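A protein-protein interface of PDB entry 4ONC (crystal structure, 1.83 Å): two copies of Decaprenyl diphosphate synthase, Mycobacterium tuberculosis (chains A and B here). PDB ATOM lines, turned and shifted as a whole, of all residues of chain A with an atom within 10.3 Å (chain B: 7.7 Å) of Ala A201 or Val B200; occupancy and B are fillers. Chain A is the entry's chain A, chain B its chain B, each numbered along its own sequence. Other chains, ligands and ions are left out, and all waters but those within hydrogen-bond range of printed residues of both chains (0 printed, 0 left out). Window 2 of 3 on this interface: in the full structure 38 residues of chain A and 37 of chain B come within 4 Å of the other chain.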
ATOM      1  N   ALA A 192      35.489 -10.428 -12.811  1.00  0.00           N
ATOM      2  CA  ALA A 192      35.449 -11.722 -13.513  1.00  0.00           C
ATOM      3  C   ALA A 192      34.575 -12.721 -12.708  1.00  0.00           C
ATOM      4  O   ALA A 192      33.754 -13.451 -13.262  1.00  0.00           O
ATOM      5  CB  ALA A 192      36.846 -12.303 -13.701  1.00  0.00           C
ATOM      6  N   THR A 193      34.698 -12.672 -11.396  1.00  0.00           N
ATOM      7  CA  THR A 193      33.952 -13.560 -10.539  1.00  0.00           C
ATOM      8  C   THR A 193      32.445 -13.146 -10.605  1.00  0.00           C
ATOM      9  O   THR A 193      31.541 -14.018 -10.636  1.00  0.00           O
ATOM     10  CB  THR A 193      34.496 -13.372  -9.118  1.00  0.00           C
ATOM     11  OG1 THR A 193      35.789 -13.984  -9.074  1.00  0.00           O
ATOM     12  CG2 THR A 193      33.629 -14.082  -8.064  1.00  0.00           C
ATOM     13  N   ARG A 194      32.156 -11.843 -10.639  1.00  0.00           N
ATOM     14  CA  ARG A 194      30.734 -11.407 -10.763  1.00  0.00           C
ATOM     15  C   ARG A 194      30.148 -11.923 -12.096  1.00  0.00           C
ATOM     16  O   ARG A 194      28.942 -12.406 -12.176  1.00  0.00           O
ATOM     17  CB  ARG A 194      30.696  -9.851 -10.690  1.00  0.00           C
ATOM     18  CG  ARG A 194      29.471  -9.192 -10.192  1.00  0.00           C
ATOM     19  CD  ARG A 194      29.615  -7.666 -10.202  1.00  0.00           C
ATOM     20  NE  ARG A 194      30.182  -7.260  -8.921  1.00  0.00           N
ATOM     21  CZ  ARG A 194      31.296  -6.537  -8.783  1.00  0.00           C
ATOM     22  NH1 ARG A 194      31.981  -6.041  -9.828  1.00  0.00           N
ATOM     23  NH2 ARG A 194      31.712  -6.256  -7.569  1.00  0.00           N
ATOM     24  N   GLU A 195      30.944 -11.818 -13.169  1.00  0.00           N
ATOM     25  CA  GLU A 195      30.486 -12.295 -14.500  1.00  0.00           C
ATOM     26  C   GLU A 195      30.188 -13.779 -14.472  1.00  0.00           C
ATOM     27  O   GLU A 195      29.127 -14.197 -14.930  1.00  0.00           O
ATOM     28  CB  GLU A 195      31.554 -12.041 -15.603  1.00  0.00           C
ATOM     29  CG  GLU A 195      30.955 -11.986 -16.972  1.00  0.00           C
ATOM     30  CD  GLU A 195      30.212 -10.679 -17.113  1.00  0.00           C
ATOM     31  OE1 GLU A 195      29.026 -10.664 -16.798  1.00  0.00           O
ATOM     32  OE2 GLU A 195      30.836  -9.639 -17.435  1.00  0.00           O
ATOM     33  N   ILE A 196      31.148 -14.566 -13.989  1.00  0.00           N
ATOM     34  CA  ILE A 196      30.960 -15.972 -13.738  1.00  0.00           C
ATOM     35  C   ILE A 196      29.680 -16.192 -12.948  1.00  0.00           C
ATOM     36  O   ILE A 196      28.849 -17.062 -13.362  1.00  0.00           O
ATOM     37  CB  ILE A 196      32.219 -16.581 -13.026  1.00  0.00           C
ATOM     38  CG1 ILE A 196      33.377 -16.669 -14.075  1.00  0.00           C
ATOM     39  CG2 ILE A 196      32.009 -17.976 -12.400  1.00  0.00           C
ATOM     40  CD1 ILE A 196      34.742 -16.938 -13.426  1.00  0.00           C
ATOM     41  N   ALA A 197      29.500 -15.475 -11.832  1.00  0.00           N
ATOM     42  CA  ALA A 197      28.286 -15.613 -11.009  1.00  0.00           C
ATOM     43  C   ALA A 197      26.990 -15.334 -11.809  1.00  0.00           C
ATOM     44  O   ALA A 197      25.945 -16.063 -11.647  1.00  0.00           O
ATOM     45  CB  ALA A 197      28.359 -14.789  -9.770  1.00  0.00           C
ATOM     46  N   ARG A 198      27.016 -14.295 -12.651  1.00  0.00           N
ATOM     47  CA  ARG A 198      25.806 -13.994 -13.505  1.00  0.00           C
ATOM     48  C   ARG A 198      25.502 -15.181 -14.422  1.00  0.00           C
ATOM     49  O   ARG A 198      24.320 -15.596 -14.556  1.00  0.00           O
ATOM     50  CB  ARG A 198      26.034 -12.718 -14.349  1.00  0.00           C
ATOM     51  CG  ARG A 198      26.040 -11.481 -13.494  1.00  0.00           C
ATOM     52  CD  ARG A 198      26.306 -10.202 -14.336  1.00  0.00           C
ATOM     53  NE  ARG A 198      26.501  -9.024 -13.439  1.00  0.00           N
ATOM     54  CZ  ARG A 198      27.688  -8.380 -13.331  1.00  0.00           C
ATOM     55  NH1 ARG A 198      28.733  -8.805 -14.063  1.00  0.00           N
ATOM     56  NH2 ARG A 198      27.811  -7.292 -12.549  1.00  0.00           N
ATOM     57  N   GLU A 199      26.541 -15.751 -15.025  1.00  0.00           N
ATOM     58  CA  GLU A 199      26.397 -16.867 -15.967  1.00  0.00           C
ATOM     59  C   GLU A 199      25.869 -18.110 -15.230  1.00  0.00           C
ATOM     60  O   GLU A 199      25.011 -18.863 -15.769  1.00  0.00           O
ATOM     61  CB  GLU A 199      27.725 -17.195 -16.669  1.00  0.00           C
ATOM     62  CG  GLU A 199      28.215 -16.118 -17.621  1.00  0.00           C
ATOM     63  CD  GLU A 199      27.168 -15.733 -18.705  1.00  0.00           C
ATOM     64  OE1 GLU A 199      26.717 -16.597 -19.492  1.00  0.00           O
ATOM     65  OE2 GLU A 199      26.771 -14.537 -18.775  1.00  0.00           O
ATOM     66  N   VAL A 200      26.333 -18.307 -13.991  1.00  0.00           N
ATOM     67  CA  VAL A 200      25.816 -19.368 -13.137  1.00  0.00           C
ATOM     68  C   VAL A 200      24.343 -19.095 -12.711  1.00  0.00           C
ATOM     69  O   VAL A 200      23.511 -20.021 -12.735  1.00  0.00           O
ATOM     70  CB  VAL A 200      26.657 -19.541 -11.864  1.00  0.00           C
ATOM     71  CG1 VAL A 200      25.988 -20.495 -10.872  1.00  0.00           C
ATOM     72  CG2 VAL A 200      28.071 -20.000 -12.227  1.00  0.00           C
ATOM     73  N   ALA A 201      24.009 -17.879 -12.292  1.00  0.00           N
ATOM     74  CA  ALA A 201      22.610 -17.568 -11.877  1.00  0.00           C
ATOM     75  C   ALA A 201      21.740 -17.857 -13.082  1.00  0.00           C
ATOM     76  O   ALA A 201      20.660 -18.436 -12.913  1.00  0.00           O
ATOM     77  CB  ALA A 201      22.434 -16.126 -11.419  1.00  0.00           C
ATOM     78  N   ALA A 202      22.230 -17.572 -14.295  1.00  0.00           N
ATOM     79  CA  ALA A 202      21.429 -17.778 -15.514  1.00  0.00           C
ATOM     80  C   ALA A 202      21.291 -19.232 -15.989  1.00  0.00           C
ATOM     81  O   ALA A 202      20.676 -19.467 -17.012  1.00  0.00           O
ATOM     82  CB  ALA A 202      21.989 -16.933 -16.654  1.00  0.00           C
ATOM     83  N   GLY A 203      21.897 -20.203 -15.285  1.00  0.00           N
ATOM     84  CA  GLY A 203      22.093 -21.536 -15.811  1.00  0.00           C
ATOM     85  C   GLY A 203      22.912 -21.668 -17.053  1.00  0.00           C
ATOM     86  O   GLY A 203      22.800 -22.689 -17.702  1.00  0.00           O
ATOM     87  N   ARG A 204      23.762 -20.689 -17.430  1.00  0.00           N
ATOM     88  CA  ARG A 204      24.633 -20.937 -18.577  1.00  0.00           C
ATOM     89  C   ARG A 204      25.956 -21.574 -18.195  1.00  0.00           C
ATOM     90  O   ARG A 204      26.725 -21.966 -19.069  1.00  0.00           O
ATOM     91  CB  ARG A 204      24.866 -19.649 -19.427  1.00  0.00           C
ATOM     92  CG  ARG A 204      23.578 -18.925 -19.882  1.00  0.00           C
ATOM     93  CD  ARG A 204      23.879 -17.756 -20.846  1.00  0.00           C
ATOM     94  NE  ARG A 204      24.169 -16.540 -20.039  1.00  0.00           N
ATOM     95  CZ  ARG A 204      23.257 -15.703 -19.562  1.00  0.00           C
ATOM     96  NH1 ARG A 204      21.963 -15.874 -19.879  1.00  0.00           N
ATOM     97  NH2 ARG A 204      23.609 -14.687 -18.778  1.00  0.00           N
ATOM     98  N   LEU A 205      26.264 -21.634 -16.899  1.00  0.00           N
ATOM     99  CA  LEU A 205      27.574 -22.124 -16.475  1.00  0.00           C
ATOM    100  C   LEU A 205      27.396 -22.919 -15.215  1.00  0.00           C
ATOM    101  O   LEU A 205      26.753 -22.466 -14.272  1.00  0.00           O
ATOM    102  CB  LEU A 205      28.557 -20.974 -16.219  1.00  0.00           C
ATOM    103  CG  LEU A 205      29.938 -21.416 -15.668  1.00  0.00           C
ATOM    104  CD1 LEU A 205      30.724 -22.161 -16.706  1.00  0.00           C
ATOM    105  CD2 LEU A 205      30.736 -20.157 -15.335  1.00  0.00           C
ATOM    106  N   ASN A 206      27.999 -24.105 -15.210  1.00  0.00           N
ATOM    107  CA  ASN A 206      28.012 -25.036 -14.080  1.00  0.00           C
ATOM    108  C   ASN A 206      29.174 -24.730 -13.107  1.00  0.00           C
ATOM    109  O   ASN A 206      30.305 -24.774 -13.532  1.00  0.00           O
ATOM    110  CB  ASN A 206      28.278 -26.431 -14.709  1.00  0.00           C
ATOM    111  CG  ASN A 206      28.178 -27.579 -13.718  1.00  0.00           C
ATOM    112  OD1 ASN A 206      28.165 -27.407 -12.498  1.00  0.00           O
ATOM    113  ND2 ASN A 206      28.146 -28.800 -14.271  1.00  0.00           N
ATOM    114  N   PRO A 207      28.890 -24.455 -11.809  1.00  0.00           N
ATOM    115  CA  PRO A 207      29.970 -24.081 -10.899  1.00  0.00           C
ATOM    116  C   PRO A 207      31.076 -25.104 -10.874  1.00  0.00           C
ATOM    117  O   PRO A 207      32.257 -24.726 -10.690  1.00  0.00           O
ATOM    118  CB  PRO A 207      29.317 -24.104  -9.517  1.00  0.00           C
ATOM    119  CG  PRO A 207      27.890 -23.726  -9.798  1.00  0.00           C
ATOM    120  CD  PRO A 207      27.560 -24.339 -11.159  1.00  0.00           C
ATOM    121  N   GLU A 208      30.715 -26.394 -11.063  1.00  0.00           N
ATOM    122  CA  GLU A 208      31.729 -27.462 -10.975  1.00  0.00           C
ATOM    123  C   GLU A 208      32.656 -27.411 -12.133  1.00  0.00           C
ATOM    124  O   GLU A 208      33.671 -28.019 -12.099  1.00  0.00           O
ATOM    125  CB  GLU A 208      31.069 -28.867 -10.821  1.00  0.00           C
ATOM    126  CG  GLU A 208      30.089 -28.890  -9.665  1.00  0.00           C
ATOM    127  CD  GLU A 208      30.755 -28.443  -8.367  1.00  0.00           C
ATOM    128  OE1 GLU A 208      31.995 -28.617  -8.163  1.00  0.00           O
ATOM    129  OE2 GLU A 208      30.090 -27.800  -7.565  1.00  0.00           O
ATOM    130  N   ILE A 210      34.118 -24.640 -13.153  1.00  0.00           N
ATOM    131  CA  ILE A 210      34.940 -23.437 -13.031  1.00  0.00           C
ATOM    132  C   ILE A 210      36.411 -23.825 -12.799  1.00  0.00           C
ATOM    133  O   ILE A 210      36.703 -24.557 -11.856  1.00  0.00           O
ATOM    134  CB  ILE A 210      34.439 -22.526 -11.894  1.00  0.00           C
ATOM    135  CG1 ILE A 210      33.107 -21.841 -12.362  1.00  0.00           C
ATOM    136  CG2 ILE A 210      35.475 -21.397 -11.663  1.00  0.00           C
ATOM    137  CD1 ILE A 210      32.293 -21.227 -11.181  1.00  0.00           C
ATOM    138  N   THR B 193      36.188 -18.427  -6.071  1.00  0.00           N
ATOM    139  CA  THR B 193      35.195 -18.135  -7.103  1.00  0.00           C
ATOM    140  C   THR B 193      34.224 -19.328  -7.266  1.00  0.00           C
ATOM    141  O   THR B 193      33.015 -19.107  -7.423  1.00  0.00           O
ATOM    142  CB  THR B 193      35.909 -17.852  -8.432  1.00  0.00           C
ATOM    143  OG1 THR B 193      36.597 -16.585  -8.276  1.00  0.00           O
ATOM    144  CG2 THR B 193      34.871 -17.641  -9.679  1.00  0.00           C
ATOM    145  N   ARG B 194      34.735 -20.561  -7.195  1.00  0.00           N
ATOM    146  CA  ARG B 194      33.860 -21.729  -7.198  1.00  0.00           C
ATOM    147  C   ARG B 194      32.884 -21.726  -6.050  1.00  0.00           C
ATOM    148  O   ARG B 194      31.724 -22.025  -6.250  1.00  0.00           O
ATOM    149  CB  ARG B 194      34.709 -22.967  -7.045  1.00  0.00           C
ATOM    150  CG  ARG B 194      34.841 -23.725  -8.293  1.00  0.00           C
ATOM    151  CD  ARG B 194      35.103 -25.184  -7.911  1.00  0.00           C
ATOM    152  NE  ARG B 194      36.130 -25.633  -8.807  1.00  0.00           N
ATOM    153  CZ  ARG B 194      37.424 -25.393  -8.610  1.00  0.00           C
ATOM    154  NH1 ARG B 194      37.820 -24.776  -7.497  1.00  0.00           N
ATOM    155  NH2 ARG B 194      38.332 -25.795  -9.502  1.00  0.00           N
ATOM    156  N   GLU B 195      33.332 -21.372  -4.846  1.00  0.00           N
ATOM    157  CA  GLU B 195      32.488 -21.404  -3.695  1.00  0.00           C
ATOM    158  C   GLU B 195      31.410 -20.333  -3.805  1.00  0.00           C
ATOM    159  O   GLU B 195      30.247 -20.578  -3.540  1.00  0.00           O
ATOM    160  CB  GLU B 195      33.299 -21.154  -2.430  1.00  0.00           C
ATOM    161  CG  GLU B 195      34.068 -22.379  -2.035  1.00  0.00           C
ATOM    162  CD  GLU B 195      33.088 -23.306  -1.369  1.00  0.00           C
ATOM    163  OE1 GLU B 195      32.829 -23.019  -0.190  1.00  0.00           O
ATOM    164  OE2 GLU B 195      32.522 -24.246  -2.012  1.00  0.00           O
ATOM    165  N   ILE B 196      31.826 -19.155  -4.239  1.00  0.00           N
ATOM    166  CA  ILE B 196      30.884 -18.081  -4.498  1.00  0.00           C
ATOM    167  C   ILE B 196      29.859 -18.599  -5.531  1.00  0.00           C
ATOM    168  O   ILE B 196      28.617 -18.365  -5.313  1.00  0.00           O
ATOM    169  CB  ILE B 196      31.642 -16.865  -5.023  1.00  0.00           C
ATOM    170  CG1 ILE B 196      32.363 -16.196  -3.781  1.00  0.00           C
ATOM    171  CG2 ILE B 196      30.678 -15.894  -5.779  1.00  0.00           C
ATOM    172  CD1 ILE B 196      33.398 -15.108  -4.161  1.00  0.00           C
ATOM    173  N   ALA B 197      30.318 -19.203  -6.633  1.00  0.00           N
ATOM    174  CA  ALA B 197      29.394 -19.688  -7.685  1.00  0.00           C
ATOM    175  C   ALA B 197      28.379 -20.701  -7.119  1.00  0.00           C
ATOM    176  O   ALA B 197      27.179 -20.669  -7.499  1.00  0.00           O
ATOM    177  CB  ALA B 197      30.177 -20.332  -8.845  1.00  0.00           C
ATOM    178  N   ARG B 198      28.834 -21.562  -6.200  1.00  0.00           N
ATOM    179  CA  ARG B 198      27.936 -22.545  -5.526  1.00  0.00           C
ATOM    180  C   ARG B 198      26.870 -21.863  -4.726  1.00  0.00           C
ATOM    181  O   ARG B 198      25.678 -22.281  -4.762  1.00  0.00           O
ATOM    182  CB  ARG B 198      28.753 -23.478  -4.593  1.00  0.00           C
ATOM    183  CG  ARG B 198      29.581 -24.394  -5.450  1.00  0.00           C
ATOM    184  CD  ARG B 198      30.371 -25.341  -4.539  1.00  0.00           C
ATOM    185  NE  ARG B 198      31.221 -26.164  -5.374  1.00  0.00           N
ATOM    186  CZ  ARG B 198      32.539 -26.246  -5.218  1.00  0.00           C
ATOM    187  NH1 ARG B 198      33.133 -25.573  -4.241  1.00  0.00           N
ATOM    188  NH2 ARG B 198      33.243 -26.994  -6.045  1.00  0.00           N
ATOM    189  N   GLU B 199      27.275 -20.832  -3.976  1.00  0.00           N
ATOM    190  CA  GLU B 199      26.340 -20.037  -3.202  1.00  0.00           C
ATOM    191  C   GLU B 199      25.312 -19.351  -4.095  1.00  0.00           C
ATOM    192  O   GLU B 199      24.137 -19.266  -3.739  1.00  0.00           O
ATOM    193  CB  GLU B 199      27.082 -19.013  -2.385  1.00  0.00           C
ATOM    194  CG  GLU B 199      27.963 -19.597  -1.265  1.00  0.00           C
ATOM    195  CD  GLU B 199      27.055 -20.222  -0.227  1.00  0.00           C
ATOM    196  OE1 GLU B 199      26.498 -19.483   0.604  1.00  0.00           O
ATOM    197  OE2 GLU B 199      26.830 -21.430  -0.306  1.00  0.00           O
ATOM    198  N   VAL B 200      25.765 -18.834  -5.230  1.00  0.00           N
ATOM    199  CA  VAL B 200      24.840 -18.189  -6.225  1.00  0.00           C
ATOM    200  C   VAL B 200      23.853 -19.253  -6.743  1.00  0.00           C
ATOM    201  O   VAL B 200      22.618 -19.003  -6.654  1.00  0.00           O
ATOM    202  CB  VAL B 200      25.583 -17.514  -7.367  1.00  0.00           C
ATOM    203  CG1 VAL B 200      24.631 -17.179  -8.548  1.00  0.00           C
ATOM    204  CG2 VAL B 200      26.288 -16.269  -6.813  1.00  0.00           C
ATOM    205  N   ALA B 201      24.367 -20.383  -7.269  1.00  0.00           N
ATOM    206  CA  ALA B 201      23.530 -21.517  -7.777  1.00  0.00           C
ATOM    207  C   ALA B 201      22.494 -21.981  -6.723  1.00  0.00           C
ATOM    208  O   ALA B 201      21.429 -22.476  -7.077  1.00  0.00           O
ATOM    209  CB  ALA B 201      24.374 -22.681  -8.267  1.00  0.00           C
ATOM    210  N   ALA B 202      22.777 -21.781  -5.453  1.00  0.00           N
ATOM    211  CA  ALA B 202      21.866 -22.173  -4.376  1.00  0.00           C
ATOM    212  C   ALA B 202      20.918 -21.069  -3.939  1.00  0.00           C
ATOM    213  O   ALA B 202      20.221 -21.227  -2.911  1.00  0.00           O
ATOM    214  CB  ALA B 202      22.670 -22.660  -3.155  1.00  0.00           C
ATOM    215  N   GLY B 203      20.913 -19.943  -4.660  1.00  0.00           N
ATOM    216  CA  GLY B 203      20.012 -18.814  -4.422  1.00  0.00           C
ATOM    217  C   GLY B 203      20.352 -18.158  -3.091  1.00  0.00           C
ATOM    218  O   GLY B 203      19.540 -17.451  -2.537  1.00  0.00           O
ATOM    219  N   ARG B 204      21.555 -18.398  -2.560  1.00  0.00           N
ATOM    220  CA  ARG B 204      21.991 -17.762  -1.295  1.00  0.00           C
ATOM    221  C   ARG B 204      22.817 -16.472  -1.417  1.00  0.00           C
ATOM    222  O   ARG B 204      23.010 -15.758  -0.410  1.00  0.00           O
ATOM    223  CB  ARG B 204      22.764 -18.765  -0.423  1.00  0.00           C
ATOM    224  CG  ARG B 204      21.885 -19.891   0.143  1.00  0.00           C
ATOM    225  CD  ARG B 204      22.564 -20.656   1.310  1.00  0.00           C
ATOM    226  NE  ARG B 204      23.768 -21.362   0.858  1.00  0.00           N
ATOM    227  CZ  ARG B 204      23.761 -22.566   0.260  1.00  0.00           C
ATOM    228  NH1 ARG B 204      22.620 -23.218   0.046  1.00  0.00           N
ATOM    229  NH2 ARG B 204      24.895 -23.142  -0.128  1.00  0.00           N
ATOM    230  N   LEU B 205      23.274 -16.155  -2.627  1.00  0.00           N
ATOM    231  CA  LEU B 205      24.112 -14.946  -2.834  1.00  0.00           C
ATOM    232  C   LEU B 205      23.706 -14.414  -4.192  1.00  0.00           C
ATOM    233  O   LEU B 205      23.596 -15.154  -5.163  1.00  0.00           O
ATOM    234  CB  LEU B 205      25.609 -15.372  -2.805  1.00  0.00           C
ATOM    235  CG  LEU B 205      26.638 -14.290  -3.197  1.00  0.00           C
ATOM    236  CD1 LEU B 205      26.520 -13.070  -2.270  1.00  0.00           C
ATOM    237  CD2 LEU B 205      28.051 -14.920  -3.232  1.00  0.00           C
ATOM    238  N   ASN B 206      23.481 -13.107  -4.274  1.00  0.00           N
ATOM    239  CA  ASN B 206      23.161 -12.524  -5.520  1.00  0.00           C
ATOM    240  C   ASN B 206      24.446 -11.952  -6.160  1.00  0.00           C
ATOM    241  O   ASN B 206      25.249 -11.342  -5.428  1.00  0.00           O
ATOM    242  CB  ASN B 206      22.197 -11.377  -5.272  1.00  0.00           C
ATOM    243  CG  ASN B 206      21.777 -10.758  -6.545  1.00  0.00           C
ATOM    244  OD1 ASN B 206      22.487  -9.920  -7.120  1.00  0.00           O
ATOM    245  ND2 ASN B 206      20.622 -11.176  -7.032  1.00  0.00           N
ATOM    246  N   PRO B 207      24.629 -12.167  -7.476  1.00  0.00           N
ATOM    247  CA  PRO B 207      25.854 -11.758  -8.194  1.00  0.00           C
ATOM    248  C   PRO B 207      26.141 -10.252  -8.017  1.00  0.00           C
ATOM    249  O   PRO B 207      27.332  -9.816  -7.947  1.00  0.00           O
ATOM    250  CB  PRO B 207      25.552 -12.116  -9.659  1.00  0.00           C
ATOM    251  CG  PRO B 207      24.576 -13.281  -9.539  1.00  0.00           C
ATOM    252  CD  PRO B 207      23.765 -13.054  -8.294  1.00  0.00           C
ATOM    253  N   GLU B 208      25.083  -9.440  -7.877  1.00  0.00           N
ATOM    254  CA  GLU B 208      25.317  -7.996  -7.754  1.00  0.00           C
ATOM    255  C   GLU B 208      25.671  -7.578  -6.371  1.00  0.00           C
ATOM    256  O   GLU B 208      25.955  -6.406  -6.150  1.00  0.00           O
ATOM    257  CB  GLU B 208      24.046  -7.188  -8.217  1.00  0.00           C
ATOM    258  CG  GLU B 208      23.571  -7.619  -9.618  1.00  0.00           C
ATOM    259  CD  GLU B 208      24.665  -7.580 -10.702  1.00  0.00           C
ATOM    260  OE1 GLU B 208      25.664  -6.807 -10.646  1.00  0.00           O
ATOM    261  OE2 GLU B 208      24.553  -8.398 -11.651  1.00  0.00           O
ATOM    262  N   ILE B 210      28.249  -9.254  -4.889  1.00  0.00           N
ATOM    263  CA  ILE B 210      29.668  -9.666  -4.810  1.00  0.00           C
ATOM    264  C   ILE B 210      30.607  -8.426  -4.820  1.00  0.00           C
ATOM    265  O   ILE B 210      30.490  -7.515  -5.709  1.00  0.00           O
ATOM    266  CB  ILE B 210      30.048 -10.601  -5.976  1.00  0.00           C
ATOM    267  CG1 ILE B 210      29.283 -11.948  -5.825  1.00  0.00           C
ATOM    268  CG2 ILE B 210      31.603 -10.813  -6.077  1.00  0.00           C
ATOM    269  CD1 ILE B 210      29.361 -12.883  -6.999  1.00  0.00           C
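OE1 of Glu A208 lies within salt-bridge range of NH2 of Arg B198 (2.9 Å).
NH2 of Arg B194 is in hydrogen-bond range of O of Ile A210.
The guanidinium group of Arg A198 is in salt-bridge range of the side-chain carboxylate of Glu B208 (2.7 Å).
NH2 of Arg A194 sits at hydrogen-bond distance from O of Ile B210, at 2.6 Å.
OG1 of Thr A193 sits at hydrogen-bond distance from OG1 of Thr B193 (2.8 Å).
N of Glu A208 sits close to OD1 of Asn A206.
The side-chain carboxylate of Glu B195 is in salt-bridge range of the guanidinium group of Arg B198.
NH1 of Arg A198 is in salt-bridge range of OE1 of Glu A195.
The side-chain amide oxygen (OD1) of Asn B206 lies within hydrogen-bond range of the backbone NH (N) of Glu B208 (2.7 Å).
Among the printed residues, merely in contact across the chains: Arg A194 with Pro B207, Ile A210 with Ala B197, Ala A197 with Ile B210, Ala A197 with Val B200, Val A200 with Ala B197, Pro A207 with Arg B194, Ala A197 with Pro B207, Val A200 with Ala B201, Ala A201 with Val B200, Ile A196 with Thr B193, Pro A207 with Ala B197, Arg A198 with Pro B207 and Pro A207 with Ala B201.
Of the printed residues of chain B, Thr A193 touches Thr B193.
Of the printed residues of chain B, Val A200 touches Ala B197 and Ala B201.
Ala A201 touches one residue of chain B.
Of the printed residues of chain B, Ile A210 touches Arg B194 and Ala B197.
Of the printed residues of chain A, Thr B193 touches Thr A193 (2.8 Å) and Ile A196 (3.8 Å).
Val B200 touches just these residues of chain A: Ala A197 and Ala A201.
Of the printed residues of chain A, Ala B201 touches Val A200 and Pro A207.
Printed residues of chain A within 4 Å of Ile B210: Arg A194 and Ala A197.
The nearest residue of chain A that does not touch Val B200 is Val A200 (4.3 Å).
Of the 17 printed residues of chain B, 9 touch a printed residue of chain A.
Hydrophobic or aromatic side chains of chain A within 4 Å of the printed part of chain B: Ile A196, Ala A197, Val A200, Ala A201, Pro A207 and Ile A210.
Among the printed residues, Asp or Glu carboxylates within 4 Å of a Lys or Arg side-chain nitrogen of the other chain: Arg A198 with Glu B208 (2.7 Å) and Glu A208 with Arg B198 (2.9 Å).
Arg A194 touches Pro B207, and with the chains exchanged Pro A207 touches Arg B194.
Arg A194 touches Ile B210, and with the chains exchanged Ile A210 touches Arg B194.
Ala A197 touches Ile B210, and with the chains exchanged Ile A210 touches Ala B197.
Arg A198 touches Glu B208, and with the chains exchanged Glu A208 touches Arg B198.
Of the 18 pairs that touch across the chains among the printed residues, 15 have their exchanged pair printed and touching as well.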
